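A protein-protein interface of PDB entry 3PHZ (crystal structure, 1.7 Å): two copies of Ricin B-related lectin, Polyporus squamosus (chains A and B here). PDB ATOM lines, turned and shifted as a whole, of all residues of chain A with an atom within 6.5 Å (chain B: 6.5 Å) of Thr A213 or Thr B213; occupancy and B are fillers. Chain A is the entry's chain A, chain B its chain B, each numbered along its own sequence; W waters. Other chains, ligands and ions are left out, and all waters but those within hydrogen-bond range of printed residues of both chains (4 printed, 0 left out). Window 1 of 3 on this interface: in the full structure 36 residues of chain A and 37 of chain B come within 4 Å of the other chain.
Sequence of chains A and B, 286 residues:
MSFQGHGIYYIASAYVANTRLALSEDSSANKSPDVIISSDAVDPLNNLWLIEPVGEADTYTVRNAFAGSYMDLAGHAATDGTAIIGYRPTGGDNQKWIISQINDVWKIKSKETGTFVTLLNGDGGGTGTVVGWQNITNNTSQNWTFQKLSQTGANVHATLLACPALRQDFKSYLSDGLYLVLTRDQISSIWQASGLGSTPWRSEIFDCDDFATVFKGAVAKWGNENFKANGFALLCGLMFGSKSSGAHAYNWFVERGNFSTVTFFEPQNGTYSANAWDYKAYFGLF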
ATOM      1  N   CYS A 208      -7.887  23.652 -31.326  1.00  0.00           N
ATOM      2  CA  CYS A 208      -9.323  23.800 -31.780  1.00  0.00           C
ATOM      3  C   CYS A 208     -10.226  22.740 -31.196  1.00  0.00           C
ATOM      4  O   CYS A 208     -11.366  23.012 -30.864  1.00  0.00           O
ATOM      5  CB  CYS A 208      -9.441  23.659 -33.296  1.00  0.00           C
ATOM      6  SG  CYS A 208      -8.447  24.916 -34.074  1.00  0.00           S
ATOM      7  N   ASP A 209      -9.697  21.531 -31.041  1.00  0.00           N
ATOM      8  CA  ASP A 209     -10.540  20.491 -30.489  1.00  0.00           C
ATOM      9  C   ASP A 209     -10.903  20.806 -29.037  1.00  0.00           C
ATOM     10  O   ASP A 209     -11.993  20.472 -28.578  1.00  0.00           O
ATOM     11  CB  ASP A 209      -9.882  19.073 -30.596  1.00  0.00           C
ATOM     12  CG  ASP A 209      -8.541  18.927 -29.825  1.00  0.00           C
ATOM     13  OD1 ASP A 209      -7.725  19.886 -29.709  1.00  0.00           O
ATOM     14  OD2 ASP A 209      -8.336  17.810 -29.314  1.00  0.00           O
ATOM     15  N   ASP A 210      -9.980  21.468 -28.323  1.00  0.00           N
ATOM     16  CA  ASP A 210     -10.253  21.824 -26.955  1.00  0.00           C
ATOM     17  C   ASP A 210     -11.341  22.900 -26.859  1.00  0.00           C
ATOM     18  O   ASP A 210     -12.223  22.833 -26.018  1.00  0.00           O
ATOM     19  CB  ASP A 210      -8.955  22.296 -26.260  1.00  0.00           C
ATOM     20  CG  ASP A 210      -7.921  21.210 -26.206  1.00  0.00           C
ATOM     21  OD1 ASP A 210      -8.306  20.065 -25.866  1.00  0.00           O
ATOM     22  OD2 ASP A 210      -6.735  21.473 -26.512  1.00  0.00           O
ATOM     23  N   PHE A 211     -11.301  23.887 -27.755  1.00  0.00           N
ATOM     24  CA  PHE A 211     -12.391  24.871 -27.750  1.00  0.00           C
ATOM     25  C   PHE A 211     -13.753  24.180 -27.992  1.00  0.00           C
ATOM     26  O   PHE A 211     -14.739  24.454 -27.333  1.00  0.00           O
ATOM     27  CB  PHE A 211     -12.172  25.948 -28.831  1.00  0.00           C
ATOM     28  CG  PHE A 211     -11.134  26.954 -28.468  1.00  0.00           C
ATOM     29  CD1 PHE A 211     -11.479  28.136 -27.796  1.00  0.00           C
ATOM     30  CD2 PHE A 211      -9.787  26.696 -28.759  1.00  0.00           C
ATOM     31  CE1 PHE A 211     -10.448  29.081 -27.509  1.00  0.00           C
ATOM     32  CE2 PHE A 211      -8.783  27.561 -28.476  1.00  0.00           C
ATOM     33  CZ  PHE A 211      -9.106  28.783 -27.841  1.00  0.00           C
ATOM     34  N   ALA A 212     -13.807  23.326 -28.990  1.00  0.00           N
ATOM     35  CA  ALA A 212     -15.077  22.681 -29.347  1.00  0.00           C
ATOM     36  C   ALA A 212     -15.554  21.666 -28.315  1.00  0.00           C
ATOM     37  O   ALA A 212     -16.753  21.544 -28.072  1.00  0.00           O
ATOM     38  CB  ALA A 212     -14.916  21.971 -30.681  1.00  0.00           C
ATOM     39  N   THR A 213     -14.625  20.993 -27.656  1.00  0.00           N
ATOM     40  CA  THR A 213     -14.990  20.089 -26.559  1.00  0.00           C
ATOM     41  C   THR A 213     -15.495  20.818 -25.349  1.00  0.00           C
ATOM     42  O   THR A 213     -16.505  20.445 -24.780  1.00  0.00           O
ATOM     43  CB  THR A 213     -13.826  19.181 -26.159  1.00  0.00           C
ATOM     44  OG1 THR A 213     -13.540  18.366 -27.311  1.00  0.00           O
ATOM     45  CG2 THR A 213     -14.249  18.196 -25.029  1.00  0.00           C
ATOM     46  N   VAL A 214     -14.752  21.841 -24.952  1.00  0.00           N
ATOM     47  CA  VAL A 214     -15.133  22.652 -23.807  1.00  0.00           C
ATOM     48  C   VAL A 214     -16.532  23.279 -24.056  1.00  0.00           C
ATOM     49  O   VAL A 214     -17.408  23.241 -23.156  1.00  0.00           O
ATOM     50  CB  VAL A 214     -14.067  23.687 -23.423  1.00  0.00           C
ATOM     51  CG1 VAL A 214     -14.667  24.693 -22.394  1.00  0.00           C
ATOM     52  CG2 VAL A 214     -12.862  22.932 -22.801  1.00  0.00           C
ATOM     53  N   PHE A 215     -16.724  23.824 -25.271  1.00  0.00           N
ATOM     54  CA  PHE A 215     -18.026  24.442 -25.546  1.00  0.00           C
ATOM     55  C   PHE A 215     -19.156  23.424 -25.532  1.00  0.00           C
ATOM     56  O   PHE A 215     -20.230  23.691 -25.011  1.00  0.00           O
ATOM     57  CB  PHE A 215     -17.996  25.255 -26.860  1.00  0.00           C
ATOM     58  CG  PHE A 215     -19.240  26.102 -27.015  1.00  0.00           C
ATOM     59  CD1 PHE A 215     -19.604  27.016 -26.002  1.00  0.00           C
ATOM     60  CD2 PHE A 215     -20.118  25.884 -28.063  1.00  0.00           C
ATOM     61  CE1 PHE A 215     -20.805  27.754 -26.101  1.00  0.00           C
ATOM     62  CE2 PHE A 215     -21.319  26.600 -28.180  1.00  0.00           C
ATOM     63  CZ  PHE A 215     -21.681  27.548 -27.193  1.00  0.00           C
ATOM     64  N   LYS A 216     -18.935  22.224 -26.137  1.00  0.00           N
ATOM     65  CA  LYS A 216     -19.967  21.194 -26.046  1.00  0.00           C
ATOM     66  C   LYS A 216     -20.335  20.836 -24.590  1.00  0.00           C
ATOM     67  O   LYS A 216     -21.530  20.727 -24.253  1.00  0.00           O
ATOM     68  CB  LYS A 216     -19.508  19.951 -26.810  1.00  0.00           C
ATOM     69  CG  LYS A 216     -20.591  18.869 -26.786  1.00  0.00           C
ATOM     70  CD  LYS A 216     -20.236  17.824 -27.806  1.00  0.00           C
ATOM     71  CE  LYS A 216     -21.269  16.604 -27.633  1.00  0.00           C
ATOM     72  NZ  LYS A 216     -22.812  17.045 -27.457  1.00  0.00           N
ATOM     73  N   GLY A 217     -19.329  20.703 -23.719  1.00  0.00           N
ATOM     74  CA  GLY A 217     -19.568  20.501 -22.309  1.00  0.00           C
ATOM     75  C   GLY A 217     -20.322  21.657 -21.672  1.00  0.00           C
ATOM     76  O   GLY A 217     -21.184  21.443 -20.835  1.00  0.00           O
ATOM     77  N   ALA A 218     -19.989  22.877 -22.066  1.00  0.00           N
ATOM     78  CA  ALA A 218     -20.676  24.039 -21.497  1.00  0.00           C
ATOM     79  C   ALA A 218     -22.159  24.099 -21.862  1.00  0.00           C
ATOM     80  O   ALA A 218     -22.960  24.479 -21.021  1.00  0.00           O
ATOM     81  CB  ALA A 218     -19.986  25.344 -21.951  1.00  0.00           C
ATOM     82  N   ALA A 220     -23.927  21.383 -22.452  1.00  0.00           N
ATOM     83  CA  ALA A 220     -24.573  20.295 -21.707  1.00  0.00           C
ATOM     84  C   ALA A 220     -24.825  20.771 -20.238  1.00  0.00           C
ATOM     85  O   ALA A 220     -25.856  20.479 -19.640  1.00  0.00           O
ATOM     86  CB  ALA A 220     -23.714  19.031 -21.715  1.00  0.00           C
ATOM     87  N   LEU A 238     -20.035  18.247 -32.615  1.00  0.00           N
ATOM     88  CA  LEU A 238     -18.635  18.533 -32.860  1.00  0.00           C
ATOM     89  C   LEU A 238     -18.324  18.038 -34.269  1.00  0.00           C
ATOM     90  O   LEU A 238     -18.932  17.061 -34.708  1.00  0.00           O
ATOM     91  CB  LEU A 238     -17.874  17.722 -31.771  1.00  0.00           C
ATOM     92  CG  LEU A 238     -16.432  17.411 -31.740  1.00  0.00           C
ATOM     93  CD1 LEU A 238     -15.580  18.680 -31.864  1.00  0.00           C
ATOM     94  CD2 LEU A 238     -16.412  16.901 -30.270  1.00  0.00           C
ATOM     95  N   PHE A 240     -14.695  17.727 -37.084  1.00  0.00           N
ATOM     96  CA  PHE A 240     -13.285  18.008 -37.434  1.00  0.00           C
ATOM     97  C   PHE A 240     -13.256  18.126 -38.938  1.00  0.00           C
ATOM     98  O   PHE A 240     -13.941  17.365 -39.643  1.00  0.00           O
ATOM     99  CB  PHE A 240     -12.337  16.851 -37.081  1.00  0.00           C
ATOM    100  CG  PHE A 240     -12.215  16.536 -35.602  1.00  0.00           C
ATOM    101  CD1 PHE A 240     -12.642  17.431 -34.602  1.00  0.00           C
ATOM    102  CD2 PHE A 240     -11.590  15.337 -35.214  1.00  0.00           C
ATOM    103  CE1 PHE A 240     -12.496  17.124 -33.236  1.00  0.00           C
ATOM    104  CE2 PHE A 240     -11.425  14.999 -33.838  1.00  0.00           C
ATOM    105  CZ  PHE A 240     -11.882  15.896 -32.852  1.00  0.00           C
ATOM    106  N   ASN A 251     -18.120  23.513 -33.644  1.00  0.00           N
ATOM    107  CA  ASN A 251     -19.346  22.949 -33.164  1.00  0.00           C
ATOM    108  C   ASN A 251     -20.370  23.131 -34.262  1.00  0.00           C
ATOM    109  O   ASN A 251     -20.151  23.886 -35.204  1.00  0.00           O
ATOM    110  CB  ASN A 251     -19.802  23.627 -31.850  1.00  0.00           C
ATOM    111  CG  ASN A 251     -18.811  23.388 -30.731  1.00  0.00           C
ATOM    112  OD1 ASN A 251     -18.029  24.290 -30.392  1.00  0.00           O
ATOM    113  ND2 ASN A 251     -18.804  22.165 -30.161  1.00  0.00           N
ATOM    114  N   PRO A 267     -15.925  28.143 -31.748  1.00  0.00           N
ATOM    115  CA  PRO A 267     -15.965  28.442 -30.317  1.00  0.00           C
ATOM    116  C   PRO A 267     -14.755  29.309 -29.863  1.00  0.00           C
ATOM    117  O   PRO A 267     -14.738  29.768 -28.740  1.00  0.00           O
ATOM    118  CB  PRO A 267     -16.028  27.009 -29.670  1.00  0.00           C
ATOM    119  CG  PRO A 267     -15.306  26.162 -30.679  1.00  0.00           C
ATOM    120  CD  PRO A 267     -15.821  26.690 -31.995  1.00  0.00           C
ATOM    121  N   LEU A 285     -19.648  14.266 -34.246  1.00  0.00           N
ATOM    122  CA  LEU A 285     -20.341  13.547 -33.192  1.00  0.00           C
ATOM    123  C   LEU A 285     -21.439  14.457 -32.675  1.00  0.00           C
ATOM    124  O   LEU A 285     -21.280  15.689 -32.756  1.00  0.00           O
ATOM    125  CB  LEU A 285     -19.317  13.307 -32.078  1.00  0.00           C
ATOM    126  CG  LEU A 285     -19.658  12.802 -30.717  1.00  0.00           C
ATOM    127  CD1 LEU A 285     -20.397  11.458 -30.885  1.00  0.00           C
ATOM    128  CD2 LEU A 285     -18.297  12.602 -29.995  1.00  0.00           C
ATOM    129  N   CYS B 208     -24.475   9.970 -19.951  1.00  0.00           N
ATOM    130  CA  CYS B 208     -23.070   9.529 -19.759  1.00  0.00           C
ATOM    131  C   CYS B 208     -22.111  10.283 -20.684  1.00  0.00           C
ATOM    132  O   CYS B 208     -20.979  10.549 -20.303  1.00  0.00           O
ATOM    133  CB  CYS B 208     -22.852   8.036 -20.017  1.00  0.00           C
ATOM    134  SG  CYS B 208     -23.802   7.145 -18.841  1.00  0.00           S
ATOM    135  N   ASP B 209     -22.548  10.536 -21.906  1.00  0.00           N
ATOM    136  CA  ASP B 209     -21.717  11.317 -22.836  1.00  0.00           C
ATOM    137  C   ASP B 209     -21.409  12.724 -22.283  1.00  0.00           C
ATOM    138  O   ASP B 209     -20.317  13.242 -22.542  1.00  0.00           O
ATOM    139  CB  ASP B 209     -22.330  11.424 -24.239  1.00  0.00           C
ATOM    140  CG  ASP B 209     -23.712  12.112 -24.271  1.00  0.00           C
ATOM    141  OD1 ASP B 209     -24.540  12.057 -23.294  1.00  0.00           O
ATOM    142  OD2 ASP B 209     -23.942  12.737 -25.345  1.00  0.00           O
ATOM    143  N   ASP B 210     -22.361  13.326 -21.563  1.00  0.00           N
ATOM    144  CA  ASP B 210     -22.147  14.652 -20.999  1.00  0.00           C
ATOM    145  C   ASP B 210     -21.104  14.587 -19.918  1.00  0.00           C
ATOM    146  O   ASP B 210     -20.203  15.424 -19.873  1.00  0.00           O
ATOM    147  CB  ASP B 210     -23.444  15.233 -20.506  1.00  0.00           C
ATOM    148  CG  ASP B 210     -24.436  15.362 -21.630  1.00  0.00           C
ATOM    149  OD1 ASP B 210     -24.052  15.833 -22.729  1.00  0.00           O
ATOM    150  OD2 ASP B 210     -25.642  15.094 -21.374  1.00  0.00           O
ATOM    151  N   PHE B 211     -21.105  13.526 -19.113  1.00  0.00           N
ATOM    152  CA  PHE B 211     -20.052  13.417 -18.075  1.00  0.00           C
ATOM    153  C   PHE B 211     -18.689  13.278 -18.761  1.00  0.00           C
ATOM    154  O   PHE B 211     -17.698  13.892 -18.334  1.00  0.00           O
ATOM    155  CB  PHE B 211     -20.275  12.173 -17.191  1.00  0.00           C
ATOM    156  CG  PHE B 211     -21.339  12.349 -16.145  1.00  0.00           C
ATOM    157  CD1 PHE B 211     -21.011  12.825 -14.860  1.00  0.00           C
ATOM    158  CD2 PHE B 211     -22.688  12.085 -16.458  1.00  0.00           C
ATOM    159  CE1 PHE B 211     -21.978  13.008 -13.876  1.00  0.00           C
ATOM    160  CE2 PHE B 211     -23.685  12.258 -15.477  1.00  0.00           C
ATOM    161  CZ  PHE B 211     -23.339  12.734 -14.169  1.00  0.00           C
ATOM    162  N   ALA B 212     -18.617  12.442 -19.817  1.00  0.00           N
ATOM    163  CA  ALA B 212     -17.307  12.162 -20.394  1.00  0.00           C
ATOM    164  C   ALA B 212     -16.797  13.390 -21.172  1.00  0.00           C
ATOM    165  O   ALA B 212     -15.598  13.624 -21.215  1.00  0.00           O
ATOM    166  CB  ALA B 212     -17.367  10.952 -21.351  1.00  0.00           C
ATOM    167  N   THR B 213     -17.723  14.152 -21.768  1.00  0.00           N
ATOM    168  CA  THR B 213     -17.336  15.322 -22.595  1.00  0.00           C
ATOM    169  C   THR B 213     -16.893  16.417 -21.640  1.00  0.00           C
ATOM    170  O   THR B 213     -15.893  17.087 -21.883  1.00  0.00           O
ATOM    171  CB  THR B 213     -18.567  15.782 -23.441  1.00  0.00           C
ATOM    172  OG1 THR B 213     -18.797  14.778 -24.454  1.00  0.00           O
ATOM    173  CG2 THR B 213     -18.240  17.088 -24.203  1.00  0.00           C
ATOM    174  N   VAL B 214     -17.694  16.670 -20.581  1.00  0.00           N
ATOM    175  CA  VAL B 214     -17.338  17.718 -19.602  1.00  0.00           C
ATOM    176  C   VAL B 214     -15.978  17.372 -18.952  1.00  0.00           C
ATOM    177  O   VAL B 214     -15.127  18.237 -18.802  1.00  0.00           O
ATOM    178  CB  VAL B 214     -18.434  17.881 -18.542  1.00  0.00           C
ATOM    179  CG1 VAL B 214     -17.883  18.776 -17.318  1.00  0.00           C
ATOM    180  CG2 VAL B 214     -19.672  18.511 -19.163  1.00  0.00           C
ATOM    181  N   PHE B 215     -15.783  16.111 -18.585  1.00  0.00           N
ATOM    182  CA  PHE B 215     -14.493  15.754 -18.010  1.00  0.00           C
ATOM    183  C   PHE B 215     -13.313  15.947 -18.991  1.00  0.00           C
ATOM    184  O   PHE B 215     -12.253  16.440 -18.609  1.00  0.00           O
ATOM    185  CB  PHE B 215     -14.471  14.305 -17.467  1.00  0.00           C
ATOM    186  CG  PHE B 215     -13.206  14.033 -16.644  1.00  0.00           C
ATOM    187  CD1 PHE B 215     -12.966  14.801 -15.539  1.00  0.00           C
ATOM    188  CD2 PHE B 215     -12.213  13.149 -17.085  1.00  0.00           C
ATOM    189  CE1 PHE B 215     -11.793  14.642 -14.772  1.00  0.00           C
ATOM    190  CE2 PHE B 215     -11.056  12.978 -16.291  1.00  0.00           C
ATOM    191  CZ  PHE B 215     -10.882  13.715 -15.140  1.00  0.00           C
ATOM    192  N   LYS B 216     -13.477  15.513 -20.254  1.00  0.00           N
ATOM    193  CA  LYS B 216     -12.430  15.749 -21.212  1.00  0.00           C
ATOM    194  C   LYS B 216     -12.133  17.245 -21.340  1.00  0.00           C
ATOM    195  O   LYS B 216     -10.969  17.602 -21.393  1.00  0.00           O
ATOM    196  CB  LYS B 216     -12.849  15.132 -22.545  1.00  0.00           C
ATOM    197  CG  LYS B 216     -11.805  15.283 -23.640  1.00  0.00           C
ATOM    198  CD  LYS B 216     -12.220  14.403 -24.782  1.00  0.00           C
ATOM    199  CE  LYS B 216     -11.156  14.443 -25.860  1.00  0.00           C
ATOM    200  NZ  LYS B 216     -11.389  15.585 -26.732  1.00  0.00           N
ATOM    201  N   GLY B 217     -13.173  18.108 -21.362  1.00  0.00           N
ATOM    202  CA  GLY B 217     -12.992  19.585 -21.340  1.00  0.00           C
ATOM    203  C   GLY B 217     -12.274  20.055 -20.077  1.00  0.00           C
ATOM    204  O   GLY B 217     -11.438  20.943 -20.145  1.00  0.00           O
ATOM    205  N   ALA B 218     -12.596  19.455 -18.936  1.00  0.00           N
ATOM    206  CA  ALA B 218     -11.982  19.845 -17.617  1.00  0.00           C
ATOM    207  C   ALA B 218     -10.469  19.556 -17.663  1.00  0.00           C
ATOM    208  O   ALA B 218      -9.694  20.343 -17.174  1.00  0.00           O
ATOM    209  CB  ALA B 218     -12.630  19.076 -16.500  1.00  0.00           C
ATOM    210  N   ALA B 220      -8.662  19.497 -20.395  1.00  0.00           N
ATOM    211  CA  ALA B 220      -8.068  20.438 -21.364  1.00  0.00           C
ATOM    212  C   ALA B 220      -7.899  21.805 -20.645  1.00  0.00           C
ATOM    213  O   ALA B 220      -6.863  22.439 -20.759  1.00  0.00           O
ATOM    214  CB  ALA B 220      -8.939  20.620 -22.565  1.00  0.00           C
ATOM    215  N   LEU B 238     -12.131   9.687 -25.013  1.00  0.00           N
ATOM    216  CA  LEU B 238     -13.548   9.410 -24.801  1.00  0.00           C
ATOM    217  C   LEU B 238     -13.829   8.065 -25.437  1.00  0.00           C
ATOM    218  O   LEU B 238     -13.228   7.732 -26.458  1.00  0.00           O
ATOM    219  CB  LEU B 238     -14.275  10.567 -25.570  1.00  0.00           C
ATOM    220  CG  LEU B 238     -15.683  10.767 -26.038  1.00  0.00           C
ATOM    221  CD1 LEU B 238     -16.609   9.957 -25.197  1.00  0.00           C
ATOM    222  CD2 LEU B 238     -15.917  12.243 -25.652  1.00  0.00           C
ATOM    223  N   PHE B 240     -17.328   5.270 -26.272  1.00  0.00           N
ATOM    224  CA  PHE B 240     -18.696   4.750 -26.037  1.00  0.00           C
ATOM    225  C   PHE B 240     -18.656   3.242 -26.128  1.00  0.00           C
ATOM    226  O   PHE B 240     -17.945   2.679 -26.979  1.00  0.00           O
ATOM    227  CB  PHE B 240     -19.638   5.211 -27.135  1.00  0.00           C
ATOM    228  CG  PHE B 240     -19.825   6.704 -27.242  1.00  0.00           C
ATOM    229  CD1 PHE B 240     -19.473   7.605 -26.216  1.00  0.00           C
ATOM    230  CD2 PHE B 240     -20.410   7.217 -28.400  1.00  0.00           C
ATOM    231  CE1 PHE B 240     -19.659   8.977 -26.378  1.00  0.00           C
ATOM    232  CE2 PHE B 240     -20.606   8.609 -28.536  1.00  0.00           C
ATOM    233  CZ  PHE B 240     -20.212   9.478 -27.512  1.00  0.00           C
ATOM    234  N   ASN B 251     -14.167   7.881 -19.999  1.00  0.00           N
ATOM    235  CA  ASN B 251     -12.917   8.440 -20.461  1.00  0.00           C
ATOM    236  C   ASN B 251     -11.835   7.360 -20.378  1.00  0.00           C
ATOM    237  O   ASN B 251     -12.057   6.275 -19.791  1.00  0.00           O
ATOM    238  CB  ASN B 251     -12.542   9.645 -19.579  1.00  0.00           C
ATOM    239  CG  ASN B 251     -13.555  10.774 -19.714  1.00  0.00           C
ATOM    240  OD1 ASN B 251     -14.376  10.983 -18.815  1.00  0.00           O
ATOM    241  ND2 ASN B 251     -13.502  11.516 -20.846  1.00  0.00           N
ATOM    242  N   PRO B 267     -16.381   9.084 -15.251  1.00  0.00           N
ATOM    243  CA  PRO B 267     -16.438  10.428 -14.746  1.00  0.00           C
ATOM    244  C   PRO B 267     -17.676  10.722 -13.871  1.00  0.00           C
ATOM    245  O   PRO B 267     -17.724  11.787 -13.232  1.00  0.00           O
ATOM    246  CB  PRO B 267     -16.423  11.277 -16.057  1.00  0.00           C
ATOM    247  CG  PRO B 267     -17.153  10.397 -17.047  1.00  0.00           C
ATOM    248  CD  PRO B 267     -16.572   9.009 -16.712  1.00  0.00           C
ATOM    249  N   LEU B 285     -12.399   8.664 -29.161  1.00  0.00           N
ATOM    250  CA  LEU B 285     -11.573   9.700 -29.767  1.00  0.00           C
ATOM    251  C   LEU B 285     -10.562  10.178 -28.712  1.00  0.00           C
ATOM    252  O   LEU B 285     -10.773   9.953 -27.529  1.00  0.00           O
ATOM    253  CB  LEU B 285     -12.391  10.885 -30.328  1.00  0.00           C
ATOM    254  CG  LEU B 285     -13.205  11.753 -29.430  1.00  0.00           C
ATOM    255  CD1 LEU B 285     -12.311  12.523 -28.514  1.00  0.00           C
ATOM    256  CD2 LEU B 285     -13.912  12.839 -30.337  1.00  0.00           C
HETATM  257  O   HOH W   1     -21.878  16.796 -24.106  1.00  0.00           O
HETATM  258  O   HOH W   2     -10.107  15.244 -29.583  1.00  0.00           O
HETATM  259  O   HOH W   3     -16.258  19.728 -22.151  1.00  0.00           O
HETATM  260  O   HOH W   4     -10.372  18.279 -25.517  1.00  0.00           O
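Water W3 bridges the backbone carbonyl oxygen of Thr B213 and the backbone carbonyl oxygen of Thr A213. Water W1 bridges the side-chain carboxylate of Asp B210 (2.7 Å) and the side-chain amino group of Lys A216 (3.5 Å). Water W4 lies within hydrogen-bond range of the side-chain carboxylate of Asp A210 (2.8 Å) and the side-chain amino group of Lys B216 (3.1 Å). Water W2 bridges OD2 of Asp A209 (3.1 Å) and NZ of Lys B216 (3.1 Å).
The backbone NH (N) of Leu A238 sits at hydrogen-bond distance from the backbone carbonyl oxygen (O) of Leu A285 (2.8 Å). The backbone carbonyl oxygen (O) of Asp B209 lies within hydrogen-bond range of the side-chain hydroxyl (OG1) of Thr B213, at 2.9 Å. The backbone carbonyl oxygen of Asp A209 lies within hydrogen-bond range of the side-chain hydroxyl of Thr A213 (2.9 Å).
Of the 17 printed residues of chain A, 7 touch a printed residue of chain B. Among the printed residues, no Asp or Glu carboxylate lies within 4 Å of a Lys or Arg side-chain nitrogen of the other chain.
Of chain B, only Thr B213, Lys B216 and Gly B217 come within 4 Å of Thr A213. Of chain A, only Thr A213, Lys A216 and Gly A217 come within 4 Å of Thr B213. Of the printed residues of chain B, Gly A217 touches Thr B213 and Val B214. Printed residues of chain A within 4 Å of Gly B217: Thr A213 (3.8 Å) and Val A214 (3.6 Å). The nearest residue of chain B that does not touch Thr A213 is Val B214 (5.8 Å). The nearest residue of chain A that does not touch Thr B213 is Val A214 (5.8 Å).
Thr A213 touches its own counterpart, Thr B213. Thr A213 touches Lys B216, and with the chains exchanged Lys A216 touches Thr B213. Thr A213 touches Gly B217, and with the chains exchanged Gly A217 touches Thr B213. Val A214 touches Gly B217, and with the chains exchanged Gly A217 touches Val B214. 17 positions are printed for both chains. Of the 10 pairs that touch across the chains among the printed residues, 9 have their exchanged pair printed and touching as well.
Ala B220 touches Asp A210 (CB to OD1, 3.4 Å). Thr A213 touches Thr B213 (CG2 to O, 3.7 Å). Thr A213 touches Lys B216 (OG1 to NZ, 3.6 Å). N of Gly B217 touches CG2 of Thr A213 (3.8 Å). O of Gly B217 touches CG2 of Val A214, at 3.6 Å. Thr B213 touches Lys A216 (CG2 to CG, 3.9 Å). Gly A217 touches Thr B213 (N to CG2, 3.8 Å). O of Gly A217 touches CG2 of Val B214, 3.7 Å away. Asp B210 touches Ala A220. Phe B240 touches Leu A285 (CE2 to CD1, 3.7 Å).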
